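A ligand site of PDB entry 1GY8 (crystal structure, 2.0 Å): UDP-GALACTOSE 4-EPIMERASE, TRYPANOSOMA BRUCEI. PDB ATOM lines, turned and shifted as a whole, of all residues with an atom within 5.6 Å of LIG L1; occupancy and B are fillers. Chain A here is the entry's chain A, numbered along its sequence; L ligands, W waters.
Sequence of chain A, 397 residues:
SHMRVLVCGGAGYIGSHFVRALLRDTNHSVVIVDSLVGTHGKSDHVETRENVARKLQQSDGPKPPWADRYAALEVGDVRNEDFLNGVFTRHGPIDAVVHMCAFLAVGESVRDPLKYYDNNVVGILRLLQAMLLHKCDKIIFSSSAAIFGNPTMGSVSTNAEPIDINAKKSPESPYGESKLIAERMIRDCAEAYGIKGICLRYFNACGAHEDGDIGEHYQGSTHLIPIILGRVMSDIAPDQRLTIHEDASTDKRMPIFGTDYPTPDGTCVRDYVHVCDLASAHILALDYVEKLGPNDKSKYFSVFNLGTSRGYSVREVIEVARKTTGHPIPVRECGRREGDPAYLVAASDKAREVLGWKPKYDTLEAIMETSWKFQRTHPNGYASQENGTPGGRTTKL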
ATOM      1  N   VAL A 106     -26.142  -6.986 -20.601  1.00  0.00           N
ATOM      2  CA  VAL A 106     -26.209  -6.271 -21.868  1.00  0.00           C
ATOM      3  C   VAL A 106     -27.390  -6.691 -22.731  1.00  0.00           C
ATOM      4  O   VAL A 106     -28.085  -5.844 -23.295  1.00  0.00           O
ATOM      5  CB  VAL A 106     -24.909  -6.457 -22.685  1.00  0.00           C
ATOM      6  CG1 VAL A 106     -25.117  -5.950 -24.111  1.00  0.00           C
ATOM      7  CG2 VAL A 106     -23.768  -5.693 -22.028  1.00  0.00           C
ATOM      8  N   PHE A 203     -13.175  -4.605 -18.130  1.00  0.00           N
ATOM      9  CA  PHE A 203     -13.519  -5.301 -19.344  1.00  0.00           C
ATOM     10  C   PHE A 203     -14.262  -6.566 -18.894  1.00  0.00           C
ATOM     11  O   PHE A 203     -15.257  -6.441 -18.168  1.00  0.00           O
ATOM     12  CB  PHE A 203     -12.271  -5.535 -20.185  1.00  0.00           C
ATOM     13  CG  PHE A 203     -11.919  -4.338 -21.048  1.00  0.00           C
ATOM     14  CD1 PHE A 203     -11.758  -3.081 -20.457  1.00  0.00           C
ATOM     15  CD2 PHE A 203     -11.880  -4.432 -22.432  1.00  0.00           C
ATOM     16  CE1 PHE A 203     -11.572  -1.945 -21.236  1.00  0.00           C
ATOM     17  CE2 PHE A 203     -11.688  -3.306 -23.231  1.00  0.00           C
ATOM     18  CZ  PHE A 203     -11.546  -2.051 -22.624  1.00  0.00           C
ATOM     19  N   ASN A 204     -13.839  -7.768 -19.240  1.00  0.00           N
ATOM     20  CA  ASN A 204     -14.627  -8.907 -18.767  1.00  0.00           C
ATOM     21  C   ASN A 204     -14.147  -9.522 -17.472  1.00  0.00           C
ATOM     22  O   ASN A 204     -13.240 -10.354 -17.467  1.00  0.00           O
ATOM     23  CB  ASN A 204     -14.762  -9.976 -19.864  1.00  0.00           C
ATOM     24  CG  ASN A 204     -15.727  -9.550 -20.968  1.00  0.00           C
ATOM     25  OD1 ASN A 204     -15.510  -8.543 -21.632  1.00  0.00           O
ATOM     26  ND2 ASN A 204     -16.796 -10.309 -21.132  1.00  0.00           N
ATOM     27  N   THR A 222     -25.649 -14.443 -16.354  1.00  0.00           N
ATOM     28  CA  THR A 222     -25.797 -14.153 -17.776  1.00  0.00           C
ATOM     29  C   THR A 222     -24.417 -14.127 -18.446  1.00  0.00           C
ATOM     30  O   THR A 222     -24.314 -13.950 -19.650  1.00  0.00           O
ATOM     31  CB  THR A 222     -26.472 -12.770 -18.009  1.00  0.00           C
ATOM     32  OG1 THR A 222     -25.633 -11.723 -17.501  1.00  0.00           O
ATOM     33  CG2 THR A 222     -27.818 -12.703 -17.298  1.00  0.00           C
ATOM     34  N   HIS A 223     -23.362 -14.319 -17.649  1.00  0.00           N
ATOM     35  CA  HIS A 223     -22.004 -14.276 -18.189  1.00  0.00           C
ATOM     36  C   HIS A 223     -21.449 -15.599 -18.688  1.00  0.00           C
ATOM     37  O   HIS A 223     -21.737 -16.653 -18.122  1.00  0.00           O
ATOM     38  CB  HIS A 223     -21.052 -13.652 -17.168  1.00  0.00           C
ATOM     39  CG  HIS A 223     -21.324 -12.198 -16.905  1.00  0.00           C
ATOM     40  ND1 HIS A 223     -22.028 -11.756 -15.810  1.00  0.00           N
ATOM     41  CD2 HIS A 223     -21.059 -11.102 -17.651  1.00  0.00           C
ATOM     42  CE1 HIS A 223     -22.185 -10.450 -15.884  1.00  0.00           C
ATOM     43  NE2 HIS A 223     -21.601 -10.019 -16.997  1.00  0.00           N
ATOM     44  N   LEU A 224     -20.648 -15.514 -19.740  1.00  0.00           N
ATOM     45  CA  LEU A 224     -20.047 -16.663 -20.400  1.00  0.00           C
ATOM     46  C   LEU A 224     -19.439 -17.772 -19.540  1.00  0.00           C
ATOM     47  O   LEU A 224     -19.947 -18.891 -19.499  1.00  0.00           O
ATOM     48  CB  LEU A 224     -18.992 -16.187 -21.418  1.00  0.00           C
ATOM     49  CG  LEU A 224     -18.332 -17.277 -22.270  1.00  0.00           C
ATOM     50  CD1 LEU A 224     -19.397 -18.051 -23.049  1.00  0.00           C
ATOM     51  CD2 LEU A 224     -17.330 -16.647 -23.210  1.00  0.00           C
ATOM     52  N   ILE A 225     -18.340 -17.462 -18.846  1.00  0.00           N
ATOM     53  CA  ILE A 225     -17.676 -18.466 -18.031  1.00  0.00           C
ATOM     54  C   ILE A 225     -18.570 -19.094 -16.959  1.00  0.00           C
ATOM     55  O   ILE A 225     -18.606 -20.324 -16.823  1.00  0.00           O
ATOM     56  CB  ILE A 225     -16.366 -17.893 -17.449  1.00  0.00           C
ATOM     57  CG1 ILE A 225     -15.411 -17.574 -18.622  1.00  0.00           C
ATOM     58  CG2 ILE A 225     -15.707 -18.901 -16.498  1.00  0.00           C
ATOM     59  CD1 ILE A 225     -14.101 -16.939 -18.221  1.00  0.00           C
ATOM     60  N   ILE A 227     -21.636 -19.531 -17.019  1.00  0.00           N
ATOM     61  CA  ILE A 227     -22.584 -20.386 -17.721  1.00  0.00           C
ATOM     62  C   ILE A 227     -21.907 -21.675 -18.203  1.00  0.00           C
ATOM     63  O   ILE A 227     -22.484 -22.759 -18.107  1.00  0.00           O
ATOM     64  CB  ILE A 227     -23.250 -19.632 -18.915  1.00  0.00           C
ATOM     65  CG1 ILE A 227     -24.172 -18.535 -18.367  1.00  0.00           C
ATOM     66  CG2 ILE A 227     -24.047 -20.607 -19.784  1.00  0.00           C
ATOM     67  CD1 ILE A 227     -24.751 -17.630 -19.422  1.00  0.00           C
ATOM     68  N   MET A 254     -23.436 -26.152 -24.584  1.00  0.00           N
ATOM     69  CA  MET A 254     -23.036 -24.762 -24.354  1.00  0.00           C
ATOM     70  C   MET A 254     -23.370 -23.913 -25.580  1.00  0.00           C
ATOM     71  O   MET A 254     -22.853 -24.153 -26.678  1.00  0.00           O
ATOM     72  CB  MET A 254     -21.532 -24.700 -24.057  1.00  0.00           C
ATOM     73  CG  MET A 254     -21.022 -23.309 -23.673  1.00  0.00           C
ATOM     74  SD  MET A 254     -21.936 -22.669 -22.255  1.00  0.00           S
ATOM     75  CE  MET A 254     -21.994 -20.933 -22.622  1.00  0.00           C
ATOM     76  N   PRO A 255     -24.240 -22.894 -25.407  1.00  0.00           N
ATOM     77  CA  PRO A 255     -24.701 -21.967 -26.452  1.00  0.00           C
ATOM     78  C   PRO A 255     -23.655 -20.919 -26.849  1.00  0.00           C
ATOM     79  O   PRO A 255     -23.128 -20.234 -25.967  1.00  0.00           O
ATOM     80  CB  PRO A 255     -25.919 -21.284 -25.831  1.00  0.00           C
ATOM     81  CG  PRO A 255     -26.283 -22.157 -24.652  1.00  0.00           C
ATOM     82  CD  PRO A 255     -24.960 -22.633 -24.154  1.00  0.00           C
ATOM     83  N   ILE A 256     -23.355 -20.786 -28.141  1.00  0.00           N
ATOM     84  CA  ILE A 256     -22.410 -19.778 -28.634  1.00  0.00           C
ATOM     85  C   ILE A 256     -23.267 -18.721 -29.343  1.00  0.00           C
ATOM     86  O   ILE A 256     -23.869 -19.003 -30.384  1.00  0.00           O
ATOM     87  CB  ILE A 256     -21.398 -20.380 -29.646  1.00  0.00           C
ATOM     88  CG1 ILE A 256     -20.477 -21.367 -28.935  1.00  0.00           C
ATOM     89  CG2 ILE A 256     -20.596 -19.255 -30.314  1.00  0.00           C
ATOM     90  CD1 ILE A 256     -19.417 -22.010 -29.828  1.00  0.00           C
ATOM     91  N   PHE A 257     -23.335 -17.515 -28.784  1.00  0.00           N
ATOM     92  CA  PHE A 257     -24.147 -16.457 -29.381  1.00  0.00           C
ATOM     93  C   PHE A 257     -23.487 -15.747 -30.562  1.00  0.00           C
ATOM     94  O   PHE A 257     -22.727 -14.800 -30.371  1.00  0.00           O
ATOM     95  CB  PHE A 257     -24.537 -15.409 -28.345  1.00  0.00           C
ATOM     96  CG  PHE A 257     -25.320 -15.953 -27.176  1.00  0.00           C
ATOM     97  CD1 PHE A 257     -26.081 -17.103 -27.303  1.00  0.00           C
ATOM     98  CD2 PHE A 257     -25.310 -15.287 -25.958  1.00  0.00           C
ATOM     99  CE1 PHE A 257     -26.825 -17.597 -26.230  1.00  0.00           C
ATOM    100  CE2 PHE A 257     -26.049 -15.764 -24.872  1.00  0.00           C
ATOM    101  CZ  PHE A 257     -26.815 -16.931 -25.012  1.00  0.00           C
ATOM    102  N   CYS A 268     -17.347 -13.473 -30.745  1.00  0.00           N
ATOM    103  CA  CYS A 268     -16.907 -12.285 -30.027  1.00  0.00           C
ATOM    104  C   CYS A 268     -15.613 -12.500 -29.258  1.00  0.00           C
ATOM    105  O   CYS A 268     -15.412 -13.543 -28.642  1.00  0.00           O
ATOM    106  CB  CYS A 268     -17.992 -11.833 -29.047  1.00  0.00           C
ATOM    107  SG  CYS A 268     -19.517 -11.256 -29.846  1.00  0.00           S
ATOM    108  N   ARG A 270     -13.117 -11.090 -26.244  1.00  0.00           N
ATOM    109  CA  ARG A 270     -13.167 -10.312 -25.018  1.00  0.00           C
ATOM    110  C   ARG A 270     -11.841 -10.405 -24.264  1.00  0.00           C
ATOM    111  O   ARG A 270     -11.005 -11.253 -24.558  1.00  0.00           O
ATOM    112  CB  ARG A 270     -14.314 -10.806 -24.139  1.00  0.00           C
ATOM    113  CG  ARG A 270     -15.713 -10.608 -24.735  1.00  0.00           C
ATOM    114  CD  ARG A 270     -16.105  -9.135 -24.733  1.00  0.00           C
ATOM    115  NE  ARG A 270     -17.487  -8.906 -25.157  1.00  0.00           N
ATOM    116  CZ  ARG A 270     -17.875  -8.693 -26.409  1.00  0.00           C
ATOM    117  NH1 ARG A 270     -16.974  -8.667 -27.390  1.00  0.00           N
ATOM    118  NH2 ARG A 270     -19.152  -8.496 -26.676  1.00  0.00           N
ATOM    119  N   TYR A 272     -10.508 -10.999 -20.628  1.00  0.00           N
ATOM    120  CA  TYR A 272     -10.878 -11.511 -19.314  1.00  0.00           C
ATOM    121  C   TYR A 272      -9.865 -11.144 -18.229  1.00  0.00           C
ATOM    122  O   TYR A 272      -8.750 -11.666 -18.189  1.00  0.00           O
ATOM    123  CB  TYR A 272     -11.098 -13.025 -19.395  1.00  0.00           C
ATOM    124  CG  TYR A 272     -12.232 -13.365 -20.335  1.00  0.00           C
ATOM    125  CD1 TYR A 272     -12.008 -13.515 -21.712  1.00  0.00           C
ATOM    126  CD2 TYR A 272     -13.546 -13.455 -19.862  1.00  0.00           C
ATOM    127  CE1 TYR A 272     -13.080 -13.727 -22.597  1.00  0.00           C
ATOM    128  CE2 TYR A 272     -14.607 -13.666 -20.739  1.00  0.00           C
ATOM    129  CZ  TYR A 272     -14.367 -13.792 -22.107  1.00  0.00           C
ATOM    130  OH  TYR A 272     -15.440 -13.973 -22.972  1.00  0.00           O
ATOM    131  N   VAL A 314     -15.056 -16.538 -27.962  1.00  0.00           N
ATOM    132  CA  VAL A 314     -15.933 -17.414 -27.208  1.00  0.00           C
ATOM    133  C   VAL A 314     -15.484 -18.865 -27.364  1.00  0.00           C
ATOM    134  O   VAL A 314     -15.483 -19.630 -26.394  1.00  0.00           O
ATOM    135  CB  VAL A 314     -17.402 -17.285 -27.683  1.00  0.00           C
ATOM    136  CG1 VAL A 314     -18.288 -18.264 -26.916  1.00  0.00           C
ATOM    137  CG2 VAL A 314     -17.891 -15.859 -27.474  1.00  0.00           C
ATOM    138  N   ARG A 337     -26.420 -12.255 -29.865  1.00  0.00           N
ATOM    139  CA  ARG A 337     -27.188 -11.728 -28.749  1.00  0.00           C
ATOM    140  C   ARG A 337     -27.114 -10.233 -28.996  1.00  0.00           C
ATOM    141  O   ARG A 337     -26.021  -9.655 -29.025  1.00  0.00           O
ATOM    142  CB  ARG A 337     -26.548 -12.071 -27.416  1.00  0.00           C
ATOM    143  CG  ARG A 337     -27.265 -11.424 -26.240  1.00  0.00           C
ATOM    144  CD  ARG A 337     -26.270 -10.812 -25.278  1.00  0.00           C
ATOM    145  NE  ARG A 337     -25.819 -11.758 -24.279  1.00  0.00           N
ATOM    146  CZ  ARG A 337     -24.662 -11.659 -23.617  1.00  0.00           C
ATOM    147  NH1 ARG A 337     -23.832 -10.655 -23.862  1.00  0.00           N
ATOM    148  NH2 ARG A 337     -24.367 -12.566 -22.701  1.00  0.00           N
ATOM    149  N   ASP A 340     -24.154  -6.871 -28.386  1.00  0.00           N
ATOM    150  CA  ASP A 340     -22.758  -7.277 -28.320  1.00  0.00           C
ATOM    151  C   ASP A 340     -21.808  -6.733 -29.390  1.00  0.00           C
ATOM    152  O   ASP A 340     -22.058  -6.901 -30.584  1.00  0.00           O
ATOM    153  CB  ASP A 340     -22.643  -8.812 -28.394  1.00  0.00           C
ATOM    154  CG  ASP A 340     -23.138  -9.512 -27.141  1.00  0.00           C
ATOM    155  OD1 ASP A 340     -23.388  -8.851 -26.110  1.00  0.00           O
ATOM    156  OD2 ASP A 340     -23.272 -10.751 -27.202  1.00  0.00           O
ATOM    157  N   PRO A 341     -20.726  -6.068 -28.966  1.00  0.00           N
ATOM    158  CA  PRO A 341     -19.744  -5.539 -29.914  1.00  0.00           C
ATOM    159  C   PRO A 341     -18.933  -6.766 -30.318  1.00  0.00           C
ATOM    160  O   PRO A 341     -18.851  -7.731 -29.545  1.00  0.00           O
ATOM    161  CB  PRO A 341     -18.921  -4.569 -29.070  1.00  0.00           C
ATOM    162  CG  PRO A 341     -19.907  -4.110 -28.047  1.00  0.00           C
ATOM    163  CD  PRO A 341     -20.581  -5.400 -27.655  1.00  0.00           C
ATOM    164  N   LEU A 344     -13.678  -6.477 -27.886  1.00  0.00           N
ATOM    165  CA  LEU A 344     -13.449  -5.582 -26.755  1.00  0.00           C
ATOM    166  C   LEU A 344     -12.235  -6.070 -25.953  1.00  0.00           C
ATOM    167  O   LEU A 344     -12.364  -6.950 -25.106  1.00  0.00           O
ATOM    168  CB  LEU A 344     -14.684  -5.540 -25.845  1.00  0.00           C
ATOM    169  CG  LEU A 344     -15.977  -4.927 -26.397  1.00  0.00           C
ATOM    170  CD1 LEU A 344     -17.107  -5.096 -25.385  1.00  0.00           C
ATOM    171  CD2 LEU A 344     -15.771  -3.442 -26.722  1.00  0.00           C
HETATM  172  N1  LIG L   1     -21.941 -15.676 -24.632  1.00  0.00           N
HETATM  173  C1  LIG L   1     -22.236 -16.866 -25.335  1.00  0.00           C
HETATM  174  N2  LIG L   1     -23.048 -17.840 -24.729  1.00  0.00           N
HETATM  175  C2  LIG L   1     -23.577 -17.622 -23.441  1.00  0.00           C
HETATM  176  C3  LIG L   1     -23.307 -16.446 -22.749  1.00  0.00           C
HETATM  177  C4  LIG L   1     -22.483 -15.475 -23.334  1.00  0.00           C
HETATM  178  O1  LIG L   1     -21.764 -17.065 -26.453  1.00  0.00           O
HETATM  179  O2  LIG L   1     -24.296 -18.484 -22.924  1.00  0.00           O
HETATM  180  C5  LIG L   1     -21.051 -14.662 -25.248  1.00  0.00           C
HETATM  181  C6  LIG L   1     -21.623 -13.250 -25.361  1.00  0.00           C
HETATM  182  O3  LIG L   1     -22.532 -13.167 -26.472  1.00  0.00           O
HETATM  183  C7  LIG L   1     -20.393 -12.417 -25.593  1.00  0.00           C
HETATM  184  C8  LIG L   1     -19.312 -13.095 -24.737  1.00  0.00           C
HETATM  185  O4  LIG L   1     -19.790 -14.476 -24.534  1.00  0.00           O
HETATM  186  O5  LIG L   1     -20.040 -12.478 -26.978  1.00  0.00           O
HETATM  187  C9  LIG L   1     -19.252 -12.450 -23.332  1.00  0.00           C
HETATM  188  O6  LIG L   1     -20.562 -12.292 -22.800  1.00  0.00           O
HETATM  189  P1  LIG L   1     -20.804 -11.857 -21.265  1.00  0.00           P
HETATM  190  O7  LIG L   1     -20.209 -12.995 -20.301  1.00  0.00           O
HETATM  191  O8  LIG L   1     -22.382 -11.697 -21.000  1.00  0.00           O
HETATM  192  O9  LIG L   1     -20.043 -10.474 -20.918  1.00  0.00           O
HETATM  193  P2  LIG L   1     -20.143  -9.139 -21.835  1.00  0.00           P
HETATM  194  O10 LIG L   1     -21.609  -8.991 -22.484  1.00  0.00           O
HETATM  195  O11 LIG L   1     -19.033  -9.199 -22.989  1.00  0.00           O
HETATM  196  O12 LIG L   1     -19.856  -7.875 -20.897  1.00  0.00           O
HETATM  197  P1  LG2 L   2     -23.314  -7.757  -9.213  1.00  0.00           P
HETATM  198  O1  LG2 L   2     -24.742  -7.710  -9.639  1.00  0.00           O
HETATM  199  O2  LG2 L   2     -22.837  -8.982  -8.575  1.00  0.00           O
HETATM  200  O3  LG2 L   2     -23.015  -6.501  -8.241  1.00  0.00           O
HETATM  201  C1  LG2 L   2     -23.890  -5.376  -8.201  1.00  0.00           C
HETATM  202  C2  LG2 L   2     -24.406  -5.215  -6.792  1.00  0.00           C
HETATM  203  O4  LG2 L   2     -25.132  -3.991  -6.781  1.00  0.00           O
HETATM  204  C3  LG2 L   2     -25.390  -6.338  -6.441  1.00  0.00           C
HETATM  205  O5  LG2 L   2     -25.012  -6.842  -5.151  1.00  0.00           O
HETATM  206  C4  LG2 L   2     -26.745  -5.630  -6.390  1.00  0.00           C
HETATM  207  O6  LG2 L   2     -27.541  -6.181  -5.316  1.00  0.00           O
HETATM  208  C5  LG2 L   2     -26.389  -4.163  -6.129  1.00  0.00           C
HETATM  209  N1  LG2 L   2     -27.350  -3.167  -6.591  1.00  0.00           N
HETATM  210  C6  LG2 L   2     -27.910  -3.003  -7.831  1.00  0.00           C
HETATM  211  N2  LG2 L   2     -28.739  -1.927  -7.835  1.00  0.00           N
HETATM  212  C7  LG2 L   2     -28.679  -1.445  -6.593  1.00  0.00           C
HETATM  213  C8  LG2 L   2     -29.337  -0.349  -6.065  1.00  0.00           C
HETATM  214  N3  LG2 L   2     -30.143   0.402  -6.798  1.00  0.00           N
HETATM  215  N4  LG2 L   2     -29.119  -0.011  -4.726  1.00  0.00           N
HETATM  216  C9  LG2 L   2     -28.289  -0.763  -3.965  1.00  0.00           C
HETATM  217  N5  LG2 L   2     -27.655  -1.828  -4.479  1.00  0.00           N
HETATM  218  C10 LG2 L   2     -27.836  -2.197  -5.801  1.00  0.00           C
HETATM  219  O7  LG2 L   2     -22.372  -7.410 -10.451  1.00  0.00           O
HETATM  220  P2  LG2 L   2     -20.806  -7.243 -10.655  1.00  0.00           P
HETATM  221  O8  LG2 L   2     -20.367  -8.190 -11.701  1.00  0.00           O
HETATM  222  O9  LG2 L   2     -20.168  -7.385  -9.319  1.00  0.00           O
HETATM  223  O10 LG2 L   2     -20.653  -5.744 -11.185  1.00  0.00           O
HETATM  224  C11 LG2 L   2     -20.435  -4.647 -10.294  1.00  0.00           C
HETATM  225  C12 LG2 L   2     -20.265  -3.365 -11.100  1.00  0.00           C
HETATM  226  O11 LG2 L   2     -19.248  -3.535 -12.087  1.00  0.00           O
HETATM  227  C13 LG2 L   2     -21.546  -2.944 -11.849  1.00  0.00           C
HETATM  228  O12 LG2 L   2     -21.648  -1.496 -11.862  1.00  0.00           O
HETATM  229  C14 LG2 L   2     -21.289  -3.463 -13.295  1.00  0.00           C
HETATM  230  O13 LG2 L   2     -22.050  -2.708 -14.249  1.00  0.00           O
HETATM  231  C15 LG2 L   2     -19.791  -3.225 -13.416  1.00  0.00           C
HETATM  232  N6  LG2 L   2     -19.127  -4.007 -14.467  1.00  0.00           N
HETATM  233  C16 LG2 L   2     -19.168  -5.439 -14.388  1.00  0.00           C
HETATM  234  C17 LG2 L   2     -18.509  -6.181 -15.378  1.00  0.00           C
HETATM  235  C18 LG2 L   2     -18.509  -7.742 -15.350  1.00  0.00           C
HETATM  236  O14 LG2 L   2     -17.923  -8.347 -16.230  1.00  0.00           O
HETATM  237  N7  LG2 L   2     -19.170  -8.296 -14.336  1.00  0.00           N
HETATM  238  C19 LG2 L   2     -17.821  -5.508 -16.438  1.00  0.00           C
HETATM  239  C20 LG2 L   2     -17.778  -4.068 -16.522  1.00  0.00           C
HETATM  240  C21 LG2 L   2     -18.437  -3.331 -15.519  1.00  0.00           C
HETATM  241  O   HOH W   1     -23.473  -8.322 -20.320  1.00  0.00           O
HETATM  242  O   HOH W   2     -23.813 -12.308 -29.512  1.00  0.00           O
HETATM  243  O   HOH W   3     -18.378  -8.041 -18.681  1.00  0.00           O
HETATM  244  O   HOH W   4     -26.961 -19.042 -21.941  1.00  0.00           O
HETATM  245  O   HOH W   5     -21.886  -7.393 -18.197  1.00  0.00           O
HETATM  246  O   HOH W   6     -21.380  -7.645 -24.758  1.00  0.00           O
HETATM  247  O   HOH W   7     -20.333  -5.279 -21.348  1.00  0.00           O
HETATM  248  O   HOH W   8     -24.409 -10.839 -19.636  1.00  0.00           O
HETATM  249  O   HOH W   9     -17.665 -12.299 -19.127  1.00  0.00           O
HETATM  250  O   HOH W  10     -17.575  -6.306 -21.748  1.00  0.00           O
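The guanidinium group of Arg 337 lies within salt-bridge range of the side-chain carboxylate of Asp 340 (2.9 Å).
The guanidinium group (NH2) of Arg 270 lies within hydrogen-bond range of the backbone carbonyl oxygen (O) of Pro 341 (3.0 Å).
NH2 of Arg 337 is in hydrogen-bond range of O of Thr 222 (3.4 Å).
The backbone carbonyl oxygen of Cys 268 lies within hydrogen-bond range of the backbone NH of Val 314, 3.1 Å away.
The side-chain sulfur (SG) of Cys 268 is in hydrogen-bond range of the backbone carbonyl oxygen (O) of Pro 341, 3.6 Å away.
An oxygen (O8) of LIG L1 lies close to the backbone carbonyl oxygen (O) of Thr 222 (3.3 Å).
CG2 of Val 106 touches O10 of LIG L1, 3.97 Å away.
CA of His 223 touches O7 of LIG L1, at 3.1 Å.
CD1 of Ile 227 touches O2 of LIG L1, at 3.6 Å.
Met 254 touches LIG L1 (CE to O2, 3.4 Å).
CA of Ile 256 touches O1 of LIG L1 (3.5 Å).
CG1 of Val 314 touches O1 of LIG L1, 3.7 Å away.
Hydrophobic or aromatic side chains that line LIG L1: Val 106, His 223, Leu 224, Ile 227, Met 254, Phe 257 and Val 314.
The nearest printed residue that does not touch LIG L1 is Tyr 272 (4.1 Å).
An oxygen (O7) of LIG L1 is in hydrogen-bond range of the backbone NH (N) of Leu 224.
The side-chain carboxylate (OD2) of Asp 340 sits at hydrogen-bond distance from an oxygen (O3) of LIG L1 (2.6 Å).
An oxygen (O11) of LIG L1 lies within salt-bridge range of the guanidinium group (NE) of Arg 270 (2.7 Å).
The backbone carbonyl oxygen (O) of Pro 255 is in hydrogen-bond range of a nitrogen (N2) of LIG L1.
The guanidinium group (NH2) of Arg 337 is in salt-bridge range of an oxygen (O8) of LIG L1.
N of Phe 257 lies within hydrogen-bond range of O1 of LIG L1, 2.8 Å away.
SG of Cys 268 sits close to O5 of LIG L1.
An oxygen (O11) of LIG L1 lies within hydrogen-bond range of the side-chain amide nitrogen (ND2) of Asn 204.
Water W8 bridges an oxygen (O8) of LIG L1 (2.6 Å) and the side-chain hydroxyl of Thr 222 (2.6 Å).
Water W9 lies within hydrogen-bond range of an oxygen (O7) of LIG L1 (2.9 Å) and the side-chain amide nitrogen (ND2) of Asn 204 (3.0 Å).
Water W10 bridges an oxygen (O12) of LIG L1 and the side-chain amide oxygen of Asn 204.
Water W1 bridges an oxygen (O10) of LIG L1 and the backbone NH (N) of Val 106.
Water W2 lies within hydrogen-bond range of N of Arg 337 (2.6 Å), OD2 of Asp 340 (2.8 Å), O of Phe 257 (2.9 Å) and O3 of LIG L1 (3.4 Å).
Water W5 lies within hydrogen-bond range of a ring nitrogen (NE2) of His 223 (2.9 Å) and an oxygen (O12) of LIG L1 (3.4 Å).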
